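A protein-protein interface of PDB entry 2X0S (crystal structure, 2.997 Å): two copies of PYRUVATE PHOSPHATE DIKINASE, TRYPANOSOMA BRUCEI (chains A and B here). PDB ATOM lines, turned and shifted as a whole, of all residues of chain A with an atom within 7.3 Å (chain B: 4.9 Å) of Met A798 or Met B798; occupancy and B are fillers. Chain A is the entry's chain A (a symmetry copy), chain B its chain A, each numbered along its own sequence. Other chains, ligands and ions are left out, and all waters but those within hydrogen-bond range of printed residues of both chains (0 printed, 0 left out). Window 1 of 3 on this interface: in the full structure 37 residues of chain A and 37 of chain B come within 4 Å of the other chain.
The guanidinium group of Arg A694 is in hydrogen-bond range of the backbone carbonyl oxygen of Cys B800 (3.2 Å). The backbone carbonyl oxygen of Leu B688 lies within hydrogen-bond range of the backbone NH of Ser A803, 3.1 Å away. O of Leu A688 lies close to O of Gly B801, 3.4 Å away. The backbone carbonyl oxygen (O) of Gly B801 is in hydrogen-bond range of the guanidinium group (NH1) of Arg A694 (2.6 Å). The backbone carbonyl oxygen of Gly A801 sits close to the backbone carbonyl oxygen of Leu B688 (3.4 Å). O of Gly B799 is in hydrogen-bond range of N of Arg A773 (3.0 Å).
The backbone carbonyl oxygen (O) of Leu A688 lies within hydrogen-bond range of the guanidinium group (NH1) of Arg A694 (3.1 Å). The backbone carbonyl oxygen (O) of Gln A797 sits at hydrogen-bond distance from the backbone NH (N) of Phe A802, at 2.8 Å. The backbone carbonyl oxygen (O) of Thr B796 sits close to the side-chain sulfur (SG) of Cys B800, at 3.3 Å.
Among the printed residues, merely in contact across the chains: Met A687 with Leu B688 (3.7 Å), Pro A772 with Met B798 (3.4 Å), Pro A772 with Gly B799 (3.8 Å), Met A798 with Pro B772 (3.4 Å), Met A798 with Met B798 (3.7 Å), Met A798 with Gly B801 (3.7 Å), Gly A799 with Pro B772 (3.8 Å), Gly A801 with Met B798 (3.7 Å) and Phe A802 with Leu B688 (3.8 Å).
Of chain B, only Pro B772 (3.4 Å), Met B798 (3.7 Å) and Gly B801 (3.7 Å) come within 4 Å of Met A798. Of chain A, only Pro A772, Met A798 and Gly A801 come within 4 Å of Met B798. Of the printed residues of chain B, Gly A801 touches Leu B688 and Met B798. Of the printed residues of chain A, Cys B800 touches Arg A694 (3.2 Å). Of the printed residues of chain B, Pro A772 touches Met B798 (3.4 Å) and Gly B799 (3.8 Å). Printed residues of chain B within 4 Å of Leu A688: Gly B801 (3.4 Å). Printed residues of chain A within 4 Å of Gly B799: Pro A772 and Arg A773. Asn A793 touches none of the printed residues of chain B. Leu A795 touches none of the printed residues of chain B. The nearest residue of chain A that does not touch Met B798 is Cys A800 (5.1 Å). The nearest printed residue of chain B that does not touch Gly A801 is Val B771 (5.1 Å).
Of the 13 printed residues of chain B, 6 touch a printed residue of chain A. Hydrophobic or aromatic side chains of chain A within 4 Å of the printed part of chain B: Met A687, Leu A688, Pro A772 and Met A798. Among the printed residues, no Asp or Glu carboxylate lies within 4 Å of a Lys or Arg side-chain nitrogen of the other chain.
Leu A688 touches Gly B801, and with the chains exchanged Gly A801 touches Leu B688. Pro A772 touches Met B798, and with the chains exchanged Met A798 touches Pro B772. Met A798 touches its own counterpart, Met B798. Met A798 touches Gly B801, and with the chains exchanged Gly A801 touches Met B798. Positions printed for both chains: 688, 732, 770, 771, 772, 794, 795, 796, 797, 798, 799, 800 and 801. Of the 15 pairs that touch across the chains among the printed residues, 9 have their exchanged pair printed and touching as well.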
ATOM      1  N   MET A 687     -33.659  15.715  -2.554  1.00  0.00           N
ATOM      2  CA  MET A 687     -32.985  16.802  -3.270  1.00  0.00           C
ATOM      3  C   MET A 687     -32.012  16.294  -4.323  1.00  0.00           C
ATOM      4  O   MET A 687     -31.961  16.792  -5.447  1.00  0.00           O
ATOM      5  CB  MET A 687     -32.204  17.683  -2.282  1.00  0.00           C
ATOM      6  CG  MET A 687     -31.591  18.935  -2.931  1.00  0.00           C
ATOM      7  SD  MET A 687     -30.140  19.612  -2.095  1.00  0.00           S
ATOM      8  CE  MET A 687     -30.812  20.293  -0.586  1.00  0.00           C
ATOM      9  N   LEU A 688     -31.231  15.299  -3.931  1.00  0.00           N
ATOM     10  CA  LEU A 688     -30.191  14.754  -4.773  1.00  0.00           C
ATOM     11  C   LEU A 688     -30.586  13.375  -5.283  1.00  0.00           C
ATOM     12  O   LEU A 688     -29.742  12.546  -5.596  1.00  0.00           O
ATOM     13  CB  LEU A 688     -28.902  14.681  -3.964  1.00  0.00           C
ATOM     14  CG  LEU A 688     -28.459  16.031  -3.396  1.00  0.00           C
ATOM     15  CD1 LEU A 688     -27.254  15.873  -2.482  1.00  0.00           C
ATOM     16  CD2 LEU A 688     -28.156  16.975  -4.549  1.00  0.00           C
ATOM     17  N   ARG A 694     -31.786  13.028 -14.979  1.00  0.00           N
ATOM     18  CA  ARG A 694     -31.775  11.653 -14.477  1.00  0.00           C
ATOM     19  C   ARG A 694     -33.086  10.972 -14.821  1.00  0.00           C
ATOM     20  O   ARG A 694     -33.133   9.967 -15.528  1.00  0.00           O
ATOM     21  CB  ARG A 694     -31.554  11.666 -12.962  1.00  0.00           C
ATOM     22  CG  ARG A 694     -30.318  12.483 -12.571  1.00  0.00           C
ATOM     23  CD  ARG A 694     -30.203  12.744 -11.082  1.00  0.00           C
ATOM     24  NE  ARG A 694     -29.047  13.589 -10.782  1.00  0.00           N
ATOM     25  CZ  ARG A 694     -28.647  13.918  -9.557  1.00  0.00           C
ATOM     26  NH1 ARG A 694     -29.308  13.474  -8.500  1.00  0.00           N
ATOM     27  NH2 ARG A 694     -27.589  14.695  -9.383  1.00  0.00           N
ATOM     28  N   LEU A 732     -30.759  20.261 -13.796  1.00  0.00           N
ATOM     29  CA  LEU A 732     -29.891  19.338 -13.066  1.00  0.00           C
ATOM     30  C   LEU A 732     -28.725  18.671 -13.818  1.00  0.00           C
ATOM     31  O   LEU A 732     -28.079  17.793 -13.258  1.00  0.00           O
ATOM     32  CB  LEU A 732     -30.740  18.269 -12.362  1.00  0.00           C
ATOM     33  CG  LEU A 732     -30.024  17.554 -11.220  1.00  0.00           C
ATOM     34  CD1 LEU A 732     -29.410  18.591 -10.306  1.00  0.00           C
ATOM     35  CD2 LEU A 732     -30.966  16.643 -10.452  1.00  0.00           C
ATOM     36  N   GLU A 770     -26.787  24.196 -11.986  1.00  0.00           N
ATOM     37  CA  GLU A 770     -27.101  24.155 -10.565  1.00  0.00           C
ATOM     38  C   GLU A 770     -26.218  23.168  -9.810  1.00  0.00           C
ATOM     39  O   GLU A 770     -26.014  23.319  -8.609  1.00  0.00           O
ATOM     40  CB  GLU A 770     -28.577  23.845 -10.346  1.00  0.00           C
ATOM     41  CG  GLU A 770     -29.135  22.789 -11.268  1.00  0.00           C
ATOM     42  CD  GLU A 770     -30.624  22.611 -11.077  1.00  0.00           C
ATOM     43  OE1 GLU A 770     -31.096  22.790  -9.937  1.00  0.00           O
ATOM     44  OE2 GLU A 770     -31.334  22.303 -12.059  1.00  0.00           O
ATOM     45  N   VAL A 771     -25.687  22.165 -10.509  1.00  0.00           N
ATOM     46  CA  VAL A 771     -24.711  21.256  -9.896  1.00  0.00           C
ATOM     47  C   VAL A 771     -23.298  21.814 -10.051  1.00  0.00           C
ATOM     48  O   VAL A 771     -22.910  22.258 -11.140  1.00  0.00           O
ATOM     49  CB  VAL A 771     -24.742  19.807 -10.482  1.00  0.00           C
ATOM     50  CG1 VAL A 771     -26.107  19.455 -10.980  1.00  0.00           C
ATOM     51  CG2 VAL A 771     -23.741  19.652 -11.588  1.00  0.00           C
ATOM     52  N   PRO A 772     -22.530  21.802  -8.951  1.00  0.00           N
ATOM     53  CA  PRO A 772     -21.157  22.314  -8.894  1.00  0.00           C
ATOM     54  C   PRO A 772     -20.267  21.754 -10.007  1.00  0.00           C
ATOM     55  O   PRO A 772     -19.463  22.498 -10.575  1.00  0.00           O
ATOM     56  CB  PRO A 772     -20.680  21.845  -7.516  1.00  0.00           C
ATOM     57  CG  PRO A 772     -21.923  21.785  -6.700  1.00  0.00           C
ATOM     58  CD  PRO A 772     -22.983  21.291  -7.648  1.00  0.00           C
ATOM     59  N   ARG A 773     -20.427  20.465 -10.314  1.00  0.00           N
ATOM     60  CA  ARG A 773     -19.617  19.785 -11.326  1.00  0.00           C
ATOM     61  C   ARG A 773     -19.806  20.423 -12.685  1.00  0.00           C
ATOM     62  O   ARG A 773     -18.881  20.491 -13.482  1.00  0.00           O
ATOM     63  CB  ARG A 773     -19.987  18.298 -11.440  1.00  0.00           C
ATOM     64  CG  ARG A 773     -19.170  17.609 -12.522  1.00  0.00           C
ATOM     65  CD  ARG A 773     -19.378  16.128 -12.650  1.00  0.00           C
ATOM     66  NE  ARG A 773     -18.323  15.550 -13.487  1.00  0.00           N
ATOM     67  CZ  ARG A 773     -18.272  15.667 -14.811  1.00  0.00           C
ATOM     68  NH1 ARG A 773     -19.223  16.344 -15.440  1.00  0.00           N
ATOM     69  NH2 ARG A 773     -17.281  15.118 -15.508  1.00  0.00           N
ATOM     70  N   GLY A 791     -28.734  28.331 -11.699  1.00  0.00           N
ATOM     71  CA  GLY A 791     -29.696  27.936 -10.686  1.00  0.00           C
ATOM     72  C   GLY A 791     -29.177  28.164  -9.286  1.00  0.00           C
ATOM     73  O   GLY A 791     -29.387  27.340  -8.392  1.00  0.00           O
ATOM     74  N   ASN A 793     -29.847  29.074  -6.658  1.00  0.00           N
ATOM     75  CA  ASN A 793     -30.528  28.600  -5.477  1.00  0.00           C
ATOM     76  C   ASN A 793     -30.001  27.198  -5.195  1.00  0.00           C
ATOM     77  O   ASN A 793     -29.241  26.971  -4.244  1.00  0.00           O
ATOM     78  CB  ASN A 793     -32.035  28.584  -5.697  1.00  0.00           C
ATOM     79  CG  ASN A 793     -32.775  28.130  -4.474  1.00  0.00           C
ATOM     80  OD1 ASN A 793     -32.421  28.505  -3.357  1.00  0.00           O
ATOM     81  ND2 ASN A 793     -33.794  27.305  -4.664  1.00  0.00           N
ATOM     82  N   ASP A 794     -30.384  26.273  -6.068  1.00  0.00           N
ATOM     83  CA  ASP A 794     -29.930  24.897  -5.980  1.00  0.00           C
ATOM     84  C   ASP A 794     -28.411  24.884  -5.856  1.00  0.00           C
ATOM     85  O   ASP A 794     -27.854  24.188  -5.006  1.00  0.00           O
ATOM     86  CB  ASP A 794     -30.377  24.107  -7.219  1.00  0.00           C
ATOM     87  CG  ASP A 794     -31.907  24.046  -7.372  1.00  0.00           C
ATOM     88  OD1 ASP A 794     -32.623  23.770  -6.376  1.00  0.00           O
ATOM     89  OD2 ASP A 794     -32.397  24.261  -8.504  1.00  0.00           O
ATOM     90  N   LEU A 795     -27.750  25.662  -6.708  1.00  0.00           N
ATOM     91  CA  LEU A 795     -26.293  25.694  -6.781  1.00  0.00           C
ATOM     92  C   LEU A 795     -25.663  26.179  -5.468  1.00  0.00           C
ATOM     93  O   LEU A 795     -24.471  26.007  -5.225  1.00  0.00           O
ATOM     94  CB  LEU A 795     -25.834  26.551  -7.969  1.00  0.00           C
ATOM     95  CG  LEU A 795     -24.322  26.754  -8.091  1.00  0.00           C
ATOM     96  CD1 LEU A 795     -23.657  25.500  -8.601  1.00  0.00           C
ATOM     97  CD2 LEU A 795     -23.973  27.904  -9.003  1.00  0.00           C
ATOM     98  N   THR A 796     -26.458  26.787  -4.604  1.00  0.00           N
ATOM     99  CA  THR A 796     -25.886  27.264  -3.356  1.00  0.00           C
ATOM    100  C   THR A 796     -25.983  26.163  -2.322  1.00  0.00           C
ATOM    101  O   THR A 796     -25.143  26.067  -1.426  1.00  0.00           O
ATOM    102  CB  THR A 796     -26.595  28.537  -2.837  1.00  0.00           C
ATOM    103  OG1 THR A 796     -26.310  29.645  -3.701  1.00  0.00           O
ATOM    104  CG2 THR A 796     -26.105  28.881  -1.445  1.00  0.00           C
ATOM    105  N   GLN A 797     -27.025  25.344  -2.467  1.00  0.00           N
ATOM    106  CA  GLN A 797     -27.332  24.254  -1.551  1.00  0.00           C
ATOM    107  C   GLN A 797     -26.312  23.155  -1.692  1.00  0.00           C
ATOM    108  O   GLN A 797     -25.857  22.590  -0.693  1.00  0.00           O
ATOM    109  CB  GLN A 797     -28.691  23.658  -1.878  1.00  0.00           C
ATOM    110  CG  GLN A 797     -29.869  24.605  -1.741  1.00  0.00           C
ATOM    111  CD  GLN A 797     -31.201  23.905  -1.950  1.00  0.00           C
ATOM    112  OE1 GLN A 797     -31.715  23.249  -1.036  1.00  0.00           O
ATOM    113  NE2 GLN A 797     -31.764  24.038  -3.155  1.00  0.00           N
ATOM    114  N   MET A 798     -25.981  22.821  -2.940  1.00  0.00           N
ATOM    115  CA  MET A 798     -24.938  21.835  -3.204  1.00  0.00           C
ATOM    116  C   MET A 798     -23.570  22.467  -3.018  1.00  0.00           C
ATOM    117  O   MET A 798     -22.676  21.850  -2.439  1.00  0.00           O
ATOM    118  CB  MET A 798     -25.041  21.283  -4.613  1.00  0.00           C
ATOM    119  CG  MET A 798     -26.435  20.977  -5.034  1.00  0.00           C
ATOM    120  SD  MET A 798     -26.429  19.797  -6.386  1.00  0.00           S
ATOM    121  CE  MET A 798     -27.824  20.347  -7.362  1.00  0.00           C
ATOM    122  N   GLY A 799     -23.408  23.695  -3.511  1.00  0.00           N
ATOM    123  CA  GLY A 799     -22.166  24.425  -3.332  1.00  0.00           C
ATOM    124  C   GLY A 799     -21.770  24.567  -1.872  1.00  0.00           C
ATOM    125  O   GLY A 799     -20.599  24.495  -1.522  1.00  0.00           O
ATOM    126  N   CYS A 800     -22.757  24.750  -1.007  1.00  0.00           N
ATOM    127  CA  CYS A 800     -22.492  25.043   0.395  1.00  0.00           C
ATOM    128  C   CYS A 800     -22.752  23.863   1.323  1.00  0.00           C
ATOM    129  O   CYS A 800     -22.247  23.815   2.460  1.00  0.00           O
ATOM    130  CB  CYS A 800     -23.342  26.231   0.818  1.00  0.00           C
ATOM    131  SG  CYS A 800     -22.728  27.756   0.147  1.00  0.00           S
ATOM    132  N   GLY A 801     -23.557  22.929   0.823  1.00  0.00           N
ATOM    133  CA  GLY A 801     -23.967  21.772   1.584  1.00  0.00           C
ATOM    134  C   GLY A 801     -25.103  22.123   2.509  1.00  0.00           C
ATOM    135  O   GLY A 801     -25.134  21.633   3.634  1.00  0.00           O
ATOM    136  N   PHE A 802     -26.024  22.972   2.033  1.00  0.00           N
ATOM    137  CA  PHE A 802     -27.190  23.421   2.811  1.00  0.00           C
ATOM    138  C   PHE A 802     -28.517  22.994   2.196  1.00  0.00           C
ATOM    139  O   PHE A 802     -28.876  23.455   1.107  1.00  0.00           O
ATOM    140  CB  PHE A 802     -27.208  24.939   2.929  1.00  0.00           C
ATOM    141  CG  PHE A 802     -26.025  25.514   3.651  1.00  0.00           C
ATOM    142  CD1 PHE A 802     -25.326  24.768   4.592  1.00  0.00           C
ATOM    143  CD2 PHE A 802     -25.620  26.822   3.401  1.00  0.00           C
ATOM    144  CE1 PHE A 802     -24.233  25.314   5.257  1.00  0.00           C
ATOM    145  CE2 PHE A 802     -24.536  27.376   4.064  1.00  0.00           C
ATOM    146  CZ  PHE A 802     -23.839  26.624   4.990  1.00  0.00           C
ATOM    147  N   SER A 803     -29.239  22.123   2.905  1.00  0.00           N
ATOM    148  CA  SER A 803     -30.604  21.752   2.535  1.00  0.00           C
ATOM    149  C   SER A 803     -31.509  22.852   3.042  1.00  0.00           C
ATOM    150  O   SER A 803     -31.859  22.872   4.225  1.00  0.00           O
ATOM    151  CB  SER A 803     -31.010  20.433   3.186  1.00  0.00           C
ATOM    152  OG  SER A 803     -32.388  20.199   2.988  1.00  0.00           O
ATOM    153  N   PHE A 825     -28.898  32.598   0.653  1.00  0.00           N
ATOM    154  CA  PHE A 825     -30.043  32.234  -0.184  1.00  0.00           C
ATOM    155  C   PHE A 825     -30.815  33.493  -0.584  1.00  0.00           C
ATOM    156  O   PHE A 825     -31.730  33.441  -1.409  1.00  0.00           O
ATOM    157  CB  PHE A 825     -30.956  31.194   0.497  1.00  0.00           C
ATOM    158  CG  PHE A 825     -30.377  29.786   0.542  1.00  0.00           C
ATOM    159  CD1 PHE A 825     -29.765  29.297   1.696  1.00  0.00           C
ATOM    160  CD2 PHE A 825     -30.456  28.951  -0.575  1.00  0.00           C
ATOM    161  CE1 PHE A 825     -29.243  28.006   1.728  1.00  0.00           C
ATOM    162  CE2 PHE A 825     -29.928  27.660  -0.553  1.00  0.00           C
ATOM    163  CZ  PHE A 825     -29.326  27.188   0.596  1.00  0.00           C
ATOM    164  N   ILE A 833     -19.698  30.597  -3.949  1.00  0.00           N
ATOM    165  CA  ILE A 833     -20.703  30.284  -4.964  1.00  0.00           C
ATOM    166  C   ILE A 833     -20.489  31.088  -6.247  1.00  0.00           C
ATOM    167  O   ILE A 833     -20.588  30.556  -7.349  1.00  0.00           O
ATOM    168  CB  ILE A 833     -22.111  30.568  -4.444  1.00  0.00           C
ATOM    169  CG1 ILE A 833     -22.379  29.698  -3.234  1.00  0.00           C
ATOM    170  CG2 ILE A 833     -23.140  30.325  -5.544  1.00  0.00           C
ATOM    171  CD1 ILE A 833     -21.971  28.280  -3.468  1.00  0.00           C
ATOM    172  N   LEU A 836     -17.503  29.751  -8.386  1.00  0.00           N
ATOM    173  CA  LEU A 836     -18.119  28.719  -9.226  1.00  0.00           C
ATOM    174  C   LEU A 836     -18.758  29.270 -10.500  1.00  0.00           C
ATOM    175  O   LEU A 836     -18.525  28.757 -11.603  1.00  0.00           O
ATOM    176  CB  LEU A 836     -19.200  27.996  -8.440  1.00  0.00           C
ATOM    177  CG  LEU A 836     -18.683  27.026  -7.396  1.00  0.00           C
ATOM    178  CD1 LEU A 836     -19.835  26.373  -6.680  1.00  0.00           C
ATOM    179  CD2 LEU A 836     -17.878  26.020  -8.140  1.00  0.00           C
ATOM    180  N   LEU B 688     -27.486  17.238   4.214  1.00  0.00           N
ATOM    181  CA  LEU B 688     -27.100  18.630   4.198  1.00  0.00           C
ATOM    182  C   LEU B 688     -27.763  19.380   5.344  1.00  0.00           C
ATOM    183  O   LEU B 688     -27.978  20.583   5.279  1.00  0.00           O
ATOM    184  CB  LEU B 688     -27.503  19.229   2.856  1.00  0.00           C
ATOM    185  CG  LEU B 688     -26.892  18.505   1.654  1.00  0.00           C
ATOM    186  CD1 LEU B 688     -27.442  19.052   0.346  1.00  0.00           C
ATOM    187  CD2 LEU B 688     -25.378  18.640   1.716  1.00  0.00           C
ATOM    188  N   LEU B 732     -17.050  18.755   7.520  1.00  0.00           N
ATOM    189  CA  LEU B 732     -18.056  19.595   6.873  1.00  0.00           C
ATOM    190  C   LEU B 732     -17.797  21.109   6.768  1.00  0.00           C
ATOM    191  O   LEU B 732     -18.690  21.840   6.357  1.00  0.00           O
ATOM    192  CB  LEU B 732     -19.432  19.343   7.507  1.00  0.00           C
ATOM    193  CG  LEU B 732     -20.610  19.784   6.642  1.00  0.00           C
ATOM    194  CD1 LEU B 732     -20.429  19.218   5.251  1.00  0.00           C
ATOM    195  CD2 LEU B 732     -21.936  19.347   7.239  1.00  0.00           C
ATOM    196  N   GLU B 770     -14.930  18.437   2.048  1.00  0.00           N
ATOM    197  CA  GLU B 770     -16.008  17.652   1.463  1.00  0.00           C
ATOM    198  C   GLU B 770     -17.073  18.530   0.818  1.00  0.00           C
ATOM    199  O   GLU B 770     -17.777  18.082  -0.082  1.00  0.00           O
ATOM    200  CB  GLU B 770     -16.622  16.720   2.501  1.00  0.00           C
ATOM    201  CG  GLU B 770     -16.800  17.339   3.865  1.00  0.00           C
ATOM    202  CD  GLU B 770     -17.306  16.333   4.874  1.00  0.00           C
ATOM    203  OE1 GLU B 770     -18.059  15.426   4.471  1.00  0.00           O
ATOM    204  OE2 GLU B 770     -16.948  16.431   6.068  1.00  0.00           O
ATOM    205  N   VAL B 771     -17.190  19.780   1.268  1.00  0.00           N
ATOM    206  CA  VAL B 771     -18.086  20.735   0.608  1.00  0.00           C
ATOM    207  C   VAL B 771     -17.356  21.450  -0.526  1.00  0.00           C
ATOM    208  O   VAL B 771     -16.220  21.912  -0.354  1.00  0.00           O
ATOM    209  CB  VAL B 771     -18.685  21.811   1.572  1.00  0.00           C
ATOM    210  CG1 VAL B 771     -18.807  21.279   2.964  1.00  0.00           C
ATOM    211  CG2 VAL B 771     -17.850  23.056   1.574  1.00  0.00           C
ATOM    212  N   PRO B 772     -18.007  21.531  -1.696  1.00  0.00           N
ATOM    213  CA  PRO B 772     -17.464  22.158  -2.905  1.00  0.00           C
ATOM    214  C   PRO B 772     -16.923  23.568  -2.653  1.00  0.00           C
ATOM    215  O   PRO B 772     -15.875  23.923  -3.198  1.00  0.00           O
ATOM    216  CB  PRO B 772     -18.676  22.191  -3.842  1.00  0.00           C
ATOM    217  CG  PRO B 772     -19.498  21.025  -3.417  1.00  0.00           C
ATOM    218  CD  PRO B 772     -19.352  20.976  -1.919  1.00  0.00           C
ATOM    219  N   ASP B 794     -18.241  12.258   0.283  1.00  0.00           N
ATOM    220  CA  ASP B 794     -19.181  13.345   0.487  1.00  0.00           C
ATOM    221  C   ASP B 794     -19.024  14.354  -0.645  1.00  0.00           C
ATOM    222  O   ASP B 794     -20.009  14.795  -1.237  1.00  0.00           O
ATOM    223  CB  ASP B 794     -18.934  14.016   1.846  1.00  0.00           C
ATOM    224  CG  ASP B 794     -19.124  13.056   3.033  1.00  0.00           C
ATOM    225  OD1 ASP B 794     -20.134  12.307   3.075  1.00  0.00           O
ATOM    226  OD2 ASP B 794     -18.263  13.061   3.942  1.00  0.00           O
ATOM    227  N   LEU B 795     -17.777  14.709  -0.940  1.00  0.00           N
ATOM    228  CA  LEU B 795     -17.461  15.730  -1.933  1.00  0.00           C
ATOM    229  C   LEU B 795     -17.940  15.334  -3.336  1.00  0.00           C
ATOM    230  O   LEU B 795     -18.031  16.160  -4.241  1.00  0.00           O
ATOM    231  CB  LEU B 795     -15.956  16.039  -1.925  1.00  0.00           C
ATOM    232  CG  LEU B 795     -15.479  17.017  -2.999  1.00  0.00           C
ATOM    233  CD1 LEU B 795     -15.879  18.429  -2.649  1.00  0.00           C
ATOM    234  CD2 LEU B 795     -13.984  16.962  -3.197  1.00  0.00           C
ATOM    235  N   THR B 796     -18.258  14.066  -3.531  1.00  0.00           N
ATOM    236  CA  THR B 796     -18.707  13.661  -4.853  1.00  0.00           C
ATOM    237  C   THR B 796     -20.212  13.811  -4.924  1.00  0.00           C
ATOM    238  O   THR B 796     -20.766  14.077  -5.992  1.00  0.00           O
ATOM    239  CB  THR B 796     -18.307  12.205  -5.186  1.00  0.00           C
ATOM    240  OG1 THR B 796     -16.886  12.110  -5.348  1.00  0.00           O
ATOM    241  CG2 THR B 796     -18.964  11.762  -6.478  1.00  0.00           C
ATOM    242  N   GLN B 797     -20.851  13.631  -3.768  1.00  0.00           N
ATOM    243  CA  GLN B 797     -22.300  13.679  -3.629  1.00  0.00           C
ATOM    244  C   GLN B 797     -22.793  15.091  -3.804  1.00  0.00           C
ATOM    245  O   GLN B 797     -23.809  15.323  -4.466  1.00  0.00           O
ATOM    246  CB  GLN B 797     -22.710  13.224  -2.238  1.00  0.00           C
ATOM    247  CG  GLN B 797     -22.347  11.793  -1.885  1.00  0.00           C
ATOM    248  CD  GLN B 797     -22.908  11.369  -0.538  1.00  0.00           C
ATOM    249  OE1 GLN B 797     -24.089  11.019  -0.433  1.00  0.00           O
ATOM    250  NE2 GLN B 797     -22.064  11.403   0.498  1.00  0.00           N
ATOM    251  N   MET B 798     -22.094  16.037  -3.175  1.00  0.00           N
ATOM    252  CA  MET B 798     -22.418  17.450  -3.344  1.00  0.00           C
ATOM    253  C   MET B 798     -21.882  17.948  -4.674  1.00  0.00           C
ATOM    254  O   MET B 798     -22.566  18.689  -5.379  1.00  0.00           O
ATOM    255  CB  MET B 798     -21.829  18.290  -2.228  1.00  0.00           C
ATOM    256  CG  MET B 798     -21.979  17.679  -0.878  1.00  0.00           C
ATOM    257  SD  MET B 798     -21.846  18.942   0.391  1.00  0.00           S
ATOM    258  CE  MET B 798     -21.013  18.058   1.705  1.00  0.00           C
ATOM    259  N   GLY B 799     -20.658  17.543  -5.015  1.00  0.00           N
ATOM    260  CA  GLY B 799     -20.071  17.899  -6.294  1.00  0.00           C
ATOM    261  C   GLY B 799     -20.930  17.482  -7.475  1.00  0.00           C
ATOM    262  O   GLY B 799     -21.031  18.190  -8.469  1.00  0.00           O
ATOM    263  N   CYS B 800     -21.575  16.330  -7.359  1.00  0.00           N
ATOM    264  CA  CYS B 800     -22.311  15.758  -8.478  1.00  0.00           C
ATOM    265  C   CYS B 800     -23.823  15.885  -8.340  1.00  0.00           C
ATOM    266  O   CYS B 800     -24.570  15.789  -9.332  1.00  0.00           O
ATOM    267  CB  CYS B 800     -21.927  14.293  -8.621  1.00  0.00           C
ATOM    268  SG  CYS B 800     -20.297  14.101  -9.299  1.00  0.00           S
ATOM    269  N   GLY B 801     -24.254  16.085  -7.098  1.00  0.00           N
ATOM    270  CA  GLY B 801     -25.658  16.164  -6.768  1.00  0.00           C
ATOM    271  C   GLY B 801     -26.253  14.786  -6.652  1.00  0.00           C
ATOM    272  O   GLY B 801     -27.387  14.584  -7.077  1.00  0.00           O
